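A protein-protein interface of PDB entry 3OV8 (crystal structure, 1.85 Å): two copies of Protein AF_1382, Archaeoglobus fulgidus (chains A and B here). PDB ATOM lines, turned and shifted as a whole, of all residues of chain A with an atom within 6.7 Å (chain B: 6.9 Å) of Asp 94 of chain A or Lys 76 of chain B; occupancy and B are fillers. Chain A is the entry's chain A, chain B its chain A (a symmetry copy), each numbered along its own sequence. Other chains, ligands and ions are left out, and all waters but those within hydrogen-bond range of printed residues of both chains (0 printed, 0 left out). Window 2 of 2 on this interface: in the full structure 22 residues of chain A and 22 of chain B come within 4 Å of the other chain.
The side-chain amino group (NZ) of Lys 76 of chain B lies within salt-bridge range of the side-chain carboxylate (OD1) of Asp 94 of chain A (3.0 Å). The backbone carbonyl oxygen (O) of Met 91 of chain A lies within hydrogen-bond range of the side-chain amino group (NZ) of Lys 76 of chain B, at 3.0 Å. The side-chain amino group (NZ) of Lys 76 of chain B lies close to the guanidinium group (NH1) of Arg 5 of chain A (2.8 Å).
NH1 of Arg 5 of chain A is in hydrogen-bond range of O of Met 91 of chain A, at 3.2 Å. The backbone carbonyl oxygen (O) of Met 59 of chain B lies within hydrogen-bond range of the backbone NH (N) of Thr 74 of chain B (2.9 Å). The guanidinium group of Arg 5 of chain A lies within salt-bridge range of the side-chain carboxylate of Asp 94 of chain A (3.0 Å). N of Lys 76 of chain B lies close to OG1 of Thr 74 of chain B (3.4 Å). The side-chain amino group (NZ) of Lys 76 of chain B lies within hydrogen-bond range of the backbone carbonyl oxygen (O) of Ala 57 of chain B, 2.9 Å away.
Among the printed residues, merely in contact across the chains: Arg 5 of chain A with Glu 56 of chain B (3.7 Å), Arg 5 of chain A with Ala 57 of chain B (3.7 Å), Ile 90 of chain A with Lys 76 of chain B (3.4 Å), Ile 90 of chain A with Lys 79 of chain B (3.98 Å), Ile 90 of chain A with Ile 80 of chain B (3.7 Å), Met 91 of chain A with Met 59 of chain B (3.8 Å) and Met 91 of chain A with Ile 80 of chain B (3.7 Å).
Of the printed residues of chain B, Arg 5 of chain A touches Glu 56 (3.7 Å), Ala 57 (3.7 Å) and Lys 76 (2.8 Å). Printed residues of chain B within 4 Å of Met 91 of chain A: Met 59, Lys 76 and Ile 80. Of chain B, only Lys 76 comes within 4 Å of Asp 94 of chain A. Printed residues of chain A within 4 Å of Met 59 of chain B: Met 91. Asp 75 of chain B touches none of the printed residues of chain A. Of the printed residues of chain A, Lys 76 of chain B touches Arg 5 (2.8 Å), Ile 90 (3.4 Å), Met 91 (3.0 Å) and Asp 94 (3.0 Å). Of the printed residues of chain A, Ile 80 of chain B touches Ile 90 (3.7 Å) and Met 91 (3.7 Å).
Of the 14 printed residues of chain B, 6 touch a printed residue of chain A. Printed residues of chain B that touch a printed residue of chain A: Glu 56, Ala 57, Met 59, Lys 76, Lys 79 and Ile 80. Hydrophobic or aromatic side chains of chain B that line the printed part of chain A: Ala 57, Met 59 and Ile 80. Of the 7 printed residues of chain A, 4 touch a printed residue of chain B. Along chain A the printed residues that touch a printed residue of chain B span positions 5 to 94. Among the printed residues, 10 pairs touch across the chains. Among the printed residues, Asp or Glu carboxylates within 4 Å of a Lys or Arg side-chain nitrogen of the other chain: Asp 94 of chain A with Lys 76 of chain B (3.0 Å).
No position is printed for both chains. Of the 10 pairs that touch across the chains among the printed residues, none has its exchanged pair printed and touching as well.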
ATOM      1  N   ARG A   5      -2.818 -12.551 -13.416  1.00  0.00           N
ATOM      2  CA  ARG A   5      -4.218 -12.183 -13.519  1.00  0.00           C
ATOM      3  C   ARG A   5      -4.733 -12.897 -14.754  1.00  0.00           C
ATOM      4  O   ARG A   5      -5.912 -13.236 -14.853  1.00  0.00           O
ATOM      5  CB  ARG A   5      -4.380 -10.674 -13.674  1.00  0.00           C
ATOM      6  CG  ARG A   5      -3.959  -9.869 -12.461  1.00  0.00           C
ATOM      7  CD  ARG A   5      -3.819  -8.401 -12.820  1.00  0.00           C
ATOM      8  NE  ARG A   5      -3.712  -7.555 -11.635  1.00  0.00           N
ATOM      9  CZ  ARG A   5      -3.753  -6.227 -11.662  1.00  0.00           C
ATOM     10  NH1 ARG A   5      -3.896  -5.594 -12.820  1.00  0.00           N
ATOM     11  NH2 ARG A   5      -3.654  -5.532 -10.535  1.00  0.00           N
ATOM     12  N   ASP A  89      -4.279  -6.539 -22.908  1.00  0.00           N
ATOM     13  CA  ASP A  89      -3.980  -5.110 -22.793  1.00  0.00           C
ATOM     14  C   ASP A  89      -4.748  -4.482 -21.619  1.00  0.00           C
ATOM     15  O   ASP A  89      -4.163  -3.786 -20.786  1.00  0.00           O
ATOM     16  CB  ASP A  89      -4.344  -4.359 -24.079  1.00  0.00           C
ATOM     17  CG  ASP A  89      -3.354  -4.603 -25.209  1.00  0.00           C
ATOM     18  OD1 ASP A  89      -2.222  -5.050 -24.925  1.00  0.00           O
ATOM     19  OD2 ASP A  89      -3.711  -4.333 -26.381  1.00  0.00           O
ATOM     20  N   ILE A  90      -6.059  -4.717 -21.580  1.00  0.00           N
ATOM     21  CA  ILE A  90      -6.922  -4.197 -20.508  1.00  0.00           C
ATOM     22  C   ILE A  90      -6.479  -4.669 -19.129  1.00  0.00           C
ATOM     23  O   ILE A  90      -6.429  -3.882 -18.181  1.00  0.00           O
ATOM     24  CB  ILE A  90      -8.400  -4.612 -20.713  1.00  0.00           C
ATOM     25  CG1 ILE A  90      -8.976  -3.970 -21.976  1.00  0.00           C
ATOM     26  CG2 ILE A  90      -9.249  -4.213 -19.498  1.00  0.00           C
ATOM     27  CD1 ILE A  90     -10.235  -4.641 -22.497  1.00  0.00           C
ATOM     28  N   MET A  91      -6.162  -5.955 -19.012  1.00  0.00           N
ATOM     29  CA  MET A  91      -5.748  -6.527 -17.734  1.00  0.00           C
ATOM     30  C   MET A  91      -4.470  -5.885 -17.207  1.00  0.00           C
ATOM     31  O   MET A  91      -4.325  -5.668 -16.004  1.00  0.00           O
ATOM     32  CB  MET A  91      -5.547  -8.037 -17.854  1.00  0.00           C
ATOM     33  CG  MET A  91      -5.401  -8.731 -16.514  1.00  0.00           C
ATOM     34  SD  MET A  91      -6.968  -8.816 -15.621  1.00  0.00           S
ATOM     35  CE  MET A  91      -7.757 -10.156 -16.492  1.00  0.00           C
ATOM     36  N   GLU A  92      -3.549  -5.579 -18.117  1.00  0.00           N
ATOM     37  CA  GLU A  92      -2.248  -5.022 -17.751  1.00  0.00           C
ATOM     38  C   GLU A  92      -2.251  -3.513 -17.498  1.00  0.00           C
ATOM     39  O   GLU A  92      -1.295  -2.974 -16.942  1.00  0.00           O
ATOM     40  CB  GLU A  92      -1.211  -5.352 -18.823  1.00  0.00           C
ATOM     41  CG  GLU A  92      -1.030  -6.839 -19.082  1.00  0.00           C
ATOM     42  CD  GLU A  92       0.008  -7.119 -20.158  1.00  0.00           C
ATOM     43  OE1 GLU A  92       0.458  -8.280 -20.264  1.00  0.00           O
ATOM     44  OE2 GLU A  92       0.375  -6.177 -20.897  1.00  0.00           O
ATOM     45  N   ASN A  93      -3.310  -2.828 -17.912  1.00  0.00           N
ATOM     46  CA  ASN A  93      -3.360  -1.381 -17.740  1.00  0.00           C
ATOM     47  C   ASN A  93      -4.317  -0.925 -16.639  1.00  0.00           C
ATOM     48  O   ASN A  93      -5.533  -0.885 -16.835  1.00  0.00           O
ATOM     49  CB  ASN A  93      -3.704  -0.691 -19.061  1.00  0.00           C
ATOM     50  CG  ASN A  93      -3.648   0.820 -18.957  1.00  0.00           C
ATOM     51  OD1 ASN A  93      -4.607   1.459 -18.526  1.00  0.00           O
ATOM     52  ND2 ASN A  93      -2.517   1.400 -19.353  1.00  0.00           N
ATOM     53  N   ASP A  94      -3.756  -0.584 -15.482  1.00  0.00           N
ATOM     54  CA  ASP A  94      -4.536  -0.040 -14.374  1.00  0.00           C
ATOM     55  C   ASP A  94      -4.548   1.486 -14.421  1.00  0.00           C
ATOM     56  O   ASP A  94      -3.663   2.106 -15.014  1.00  0.00           O
ATOM     57  CB  ASP A  94      -3.982  -0.518 -13.026  1.00  0.00           C
ATOM     58  CG  ASP A  94      -4.401  -1.940 -12.686  1.00  0.00           C
ATOM     59  OD1 ASP A  94      -5.534  -2.336 -13.037  1.00  0.00           O
ATOM     60  OD2 ASP A  94      -3.597  -2.661 -12.059  1.00  0.00           O
ATOM     61  N   GLU B  56      -8.514  -8.320  -6.209  1.00  0.00           N
ATOM     62  CA  GLU B  56      -7.075  -8.071  -6.309  1.00  0.00           C
ATOM     63  C   GLU B  56      -6.689  -7.552  -7.686  1.00  0.00           C
ATOM     64  O   GLU B  56      -5.814  -6.688  -7.814  1.00  0.00           O
ATOM     65  CB  GLU B  56      -6.287  -9.350  -6.018  1.00  0.00           C
ATOM     66  CG  GLU B  56      -6.484  -9.918  -4.624  1.00  0.00           C
ATOM     67  CD  GLU B  56      -5.680  -9.182  -3.573  1.00  0.00           C
ATOM     68  OE1 GLU B  56      -5.695  -7.932  -3.579  1.00  0.00           O
ATOM     69  OE2 GLU B  56      -5.026  -9.855  -2.745  1.00  0.00           O
ATOM     70  N   ALA B  57      -7.331  -8.092  -8.718  1.00  0.00           N
ATOM     71  CA  ALA B  57      -7.060  -7.695 -10.098  1.00  0.00           C
ATOM     72  C   ALA B  57      -7.809  -6.418 -10.497  1.00  0.00           C
ATOM     73  O   ALA B  57      -7.807  -6.026 -11.667  1.00  0.00           O
ATOM     74  CB  ALA B  57      -7.395  -8.832 -11.054  1.00  0.00           C
ATOM     75  N   LYS B  58      -8.448  -5.783  -9.523  1.00  0.00           N
ATOM     76  CA  LYS B  58      -9.209  -4.550  -9.750  1.00  0.00           C
ATOM     77  C   LYS B  58     -10.329  -4.696 -10.782  1.00  0.00           C
ATOM     78  O   LYS B  58     -10.652  -3.737 -11.490  1.00  0.00           O
ATOM     79  CB  LYS B  58      -8.278  -3.408 -10.170  1.00  0.00           C
ATOM     80  CG  LYS B  58      -7.016  -3.270  -9.330  1.00  0.00           C
ATOM     81  CD  LYS B  58      -7.330  -2.879  -7.897  1.00  0.00           C
ATOM     82  CE  LYS B  58      -6.054  -2.579  -7.122  1.00  0.00           C
ATOM     83  NZ  LYS B  58      -6.340  -2.230  -5.701  1.00  0.00           N
ATOM     84  N   MET B  59     -10.913  -5.890 -10.866  1.00  0.00           N
ATOM     85  CA  MET B  59     -11.993  -6.172 -11.815  1.00  0.00           C
ATOM     86  C   MET B  59     -13.376  -6.111 -11.139  1.00  0.00           C
ATOM     87  O   MET B  59     -14.388  -5.909 -11.803  1.00  0.00           O
ATOM     88  CB  MET B  59     -11.809  -7.558 -12.450  1.00  0.00           C
ATOM     89  CG  MET B  59     -10.615  -7.654 -13.391  1.00  0.00           C
ATOM     90  SD  MET B  59     -10.268  -9.374 -13.800  1.00  0.00           S
ATOM     91  CE  MET B  59     -11.749  -9.858 -14.680  1.00  0.00           C
ATOM     92  N   VAL B  60     -13.411  -6.325  -9.829  1.00  0.00           N
ATOM     93  CA  VAL B  60     -14.646  -6.139  -9.067  1.00  0.00           C
ATOM     94  C   VAL B  60     -14.351  -5.381  -7.796  1.00  0.00           C
ATOM     95  O   VAL B  60     -13.196  -5.275  -7.370  1.00  0.00           O
ATOM     96  CB  VAL B  60     -15.334  -7.483  -8.684  1.00  0.00           C
ATOM     97  CG1 VAL B  60     -15.567  -8.340  -9.903  1.00  0.00           C
ATOM     98  CG2 VAL B  60     -14.539  -8.233  -7.611  1.00  0.00           C
ATOM     99  N   LEU B  73     -18.871  -4.953 -10.814  1.00  0.00           N
ATOM    100  CA  LEU B  73     -17.739  -4.869 -11.747  1.00  0.00           C
ATOM    101  C   LEU B  73     -17.172  -3.465 -11.749  1.00  0.00           C
ATOM    102  O   LEU B  73     -17.916  -2.495 -11.714  1.00  0.00           O
ATOM    103  CB  LEU B  73     -18.177  -5.225 -13.172  1.00  0.00           C
ATOM    104  CG  LEU B  73     -18.446  -6.711 -13.409  1.00  0.00           C
ATOM    105  CD1 LEU B  73     -18.981  -6.962 -14.800  1.00  0.00           C
ATOM    106  CD2 LEU B  73     -17.174  -7.483 -13.185  1.00  0.00           C
ATOM    107  N   THR B  74     -15.851  -3.355 -11.796  1.00  0.00           N
ATOM    108  CA  THR B  74     -15.215  -2.066 -12.026  1.00  0.00           C
ATOM    109  C   THR B  74     -15.282  -1.823 -13.529  1.00  0.00           C
ATOM    110  O   THR B  74     -15.644  -2.722 -14.285  1.00  0.00           O
ATOM    111  CB  THR B  74     -13.749  -2.090 -11.595  1.00  0.00           C
ATOM    112  OG1 THR B  74     -13.050  -3.095 -12.349  1.00  0.00           O
ATOM    113  CG2 THR B  74     -13.650  -2.413 -10.091  1.00  0.00           C
ATOM    114  N   ASP B  75     -14.946  -0.619 -13.974  1.00  0.00           N
ATOM    115  CA  ASP B  75     -14.909  -0.371 -15.410  1.00  0.00           C
ATOM    116  C   ASP B  75     -14.010  -1.391 -16.099  1.00  0.00           C
ATOM    117  O   ASP B  75     -14.327  -1.876 -17.178  1.00  0.00           O
ATOM    118  CB  ASP B  75     -14.457   1.059 -15.711  1.00  0.00           C
ATOM    119  CG  ASP B  75     -15.521   2.093 -15.336  1.00  0.00           C
ATOM    120  OD1 ASP B  75     -16.722   1.732 -15.316  1.00  0.00           O
ATOM    121  OD2 ASP B  75     -15.157   3.259 -15.055  1.00  0.00           O
ATOM    122  N   LYS B  76     -12.904  -1.733 -15.451  1.00  0.00           N
ATOM    123  CA  LYS B  76     -11.962  -2.707 -15.993  1.00  0.00           C
ATOM    124  C   LYS B  76     -12.618  -4.087 -16.107  1.00  0.00           C
ATOM    125  O   LYS B  76     -12.520  -4.745 -17.140  1.00  0.00           O
ATOM    126  CB  LYS B  76     -10.723  -2.778 -15.101  1.00  0.00           C
ATOM    127  CG  LYS B  76      -9.679  -3.801 -15.524  1.00  0.00           C
ATOM    128  CD  LYS B  76      -8.551  -3.874 -14.500  1.00  0.00           C
ATOM    129  CE  LYS B  76      -7.373  -4.652 -15.055  1.00  0.00           C
ATOM    130  NZ  LYS B  76      -6.417  -5.045 -13.994  1.00  0.00           N
ATOM    131  N   GLY B  77     -13.298  -4.519 -15.051  1.00  0.00           N
ATOM    132  CA  GLY B  77     -13.950  -5.817 -15.078  1.00  0.00           C
ATOM    133  C   GLY B  77     -15.023  -5.843 -16.155  1.00  0.00           C
ATOM    134  O   GLY B  77     -15.217  -6.845 -16.835  1.00  0.00           O
ATOM    135  N   GLN B  78     -15.753  -4.745 -16.284  1.00  0.00           N
ATOM    136  CA  GLN B  78     -16.803  -4.662 -17.289  1.00  0.00           C
ATOM    137  C   GLN B  78     -16.264  -4.831 -18.715  1.00  0.00           C
ATOM    138  O   GLN B  78     -16.818  -5.589 -19.512  1.00  0.00           O
ATOM    139  CB  GLN B  78     -17.556  -3.334 -17.158  1.00  0.00           C
ATOM    140  CG  GLN B  78     -18.572  -3.115 -18.233  1.00  0.00           C
ATOM    141  CD  GLN B  78     -19.967  -3.391 -17.748  1.00  0.00           C
ATOM    142  OE1 GLN B  78     -20.158  -4.064 -16.729  1.00  0.00           O
ATOM    143  NE2 GLN B  78     -20.958  -2.862 -18.462  1.00  0.00           N
ATOM    144  N   LYS B  79     -15.186  -4.127 -19.040  1.00  0.00           N
ATOM    145  CA  LYS B  79     -14.603  -4.215 -20.381  1.00  0.00           C
ATOM    146  C   LYS B  79     -14.171  -5.651 -20.698  1.00  0.00           C
ATOM    147  O   LYS B  79     -14.392  -6.170 -21.797  1.00  0.00           O
ATOM    148  CB  LYS B  79     -13.392  -3.297 -20.477  1.00  0.00           C
ATOM    149  CG  LYS B  79     -13.703  -1.808 -20.407  1.00  0.00           C
ATOM    150  CD  LYS B  79     -12.418  -0.990 -20.496  1.00  0.00           C
ATOM    151  CE  LYS B  79     -12.679   0.494 -20.286  1.00  0.00           C
ATOM    152  NZ  LYS B  79     -11.422   1.292 -20.366  1.00  0.00           N
ATOM    153  N   ILE B  80     -13.542  -6.287 -19.721  1.00  0.00           N
ATOM    154  CA  ILE B  80     -13.082  -7.653 -19.895  1.00  0.00           C
ATOM    155  C   ILE B  80     -14.263  -8.596 -20.150  1.00  0.00           C
ATOM    156  O   ILE B  80     -14.241  -9.382 -21.092  1.00  0.00           O
ATOM    157  CB  ILE B  80     -12.254  -8.111 -18.686  1.00  0.00           C
ATOM    158  CG1 ILE B  80     -10.906  -7.371 -18.691  1.00  0.00           C
ATOM    159  CG2 ILE B  80     -12.037  -9.626 -18.722  1.00  0.00           C
ATOM    160  CD1 ILE B  80     -10.154  -7.461 -17.392  1.00  0.00           C
ATOM    161  N   ALA B  81     -15.308  -8.498 -19.326  1.00  0.00           N
ATOM    162  CA  ALA B  81     -16.485  -9.345 -19.501  1.00  0.00           C
ATOM    163  C   ALA B  81     -17.085  -9.156 -20.885  1.00  0.00           C
ATOM    164  O   ALA B  81     -17.500 -10.118 -21.533  1.00  0.00           O
ATOM    165  CB  ALA B  81     -17.551  -9.037 -18.414  1.00  0.00           C
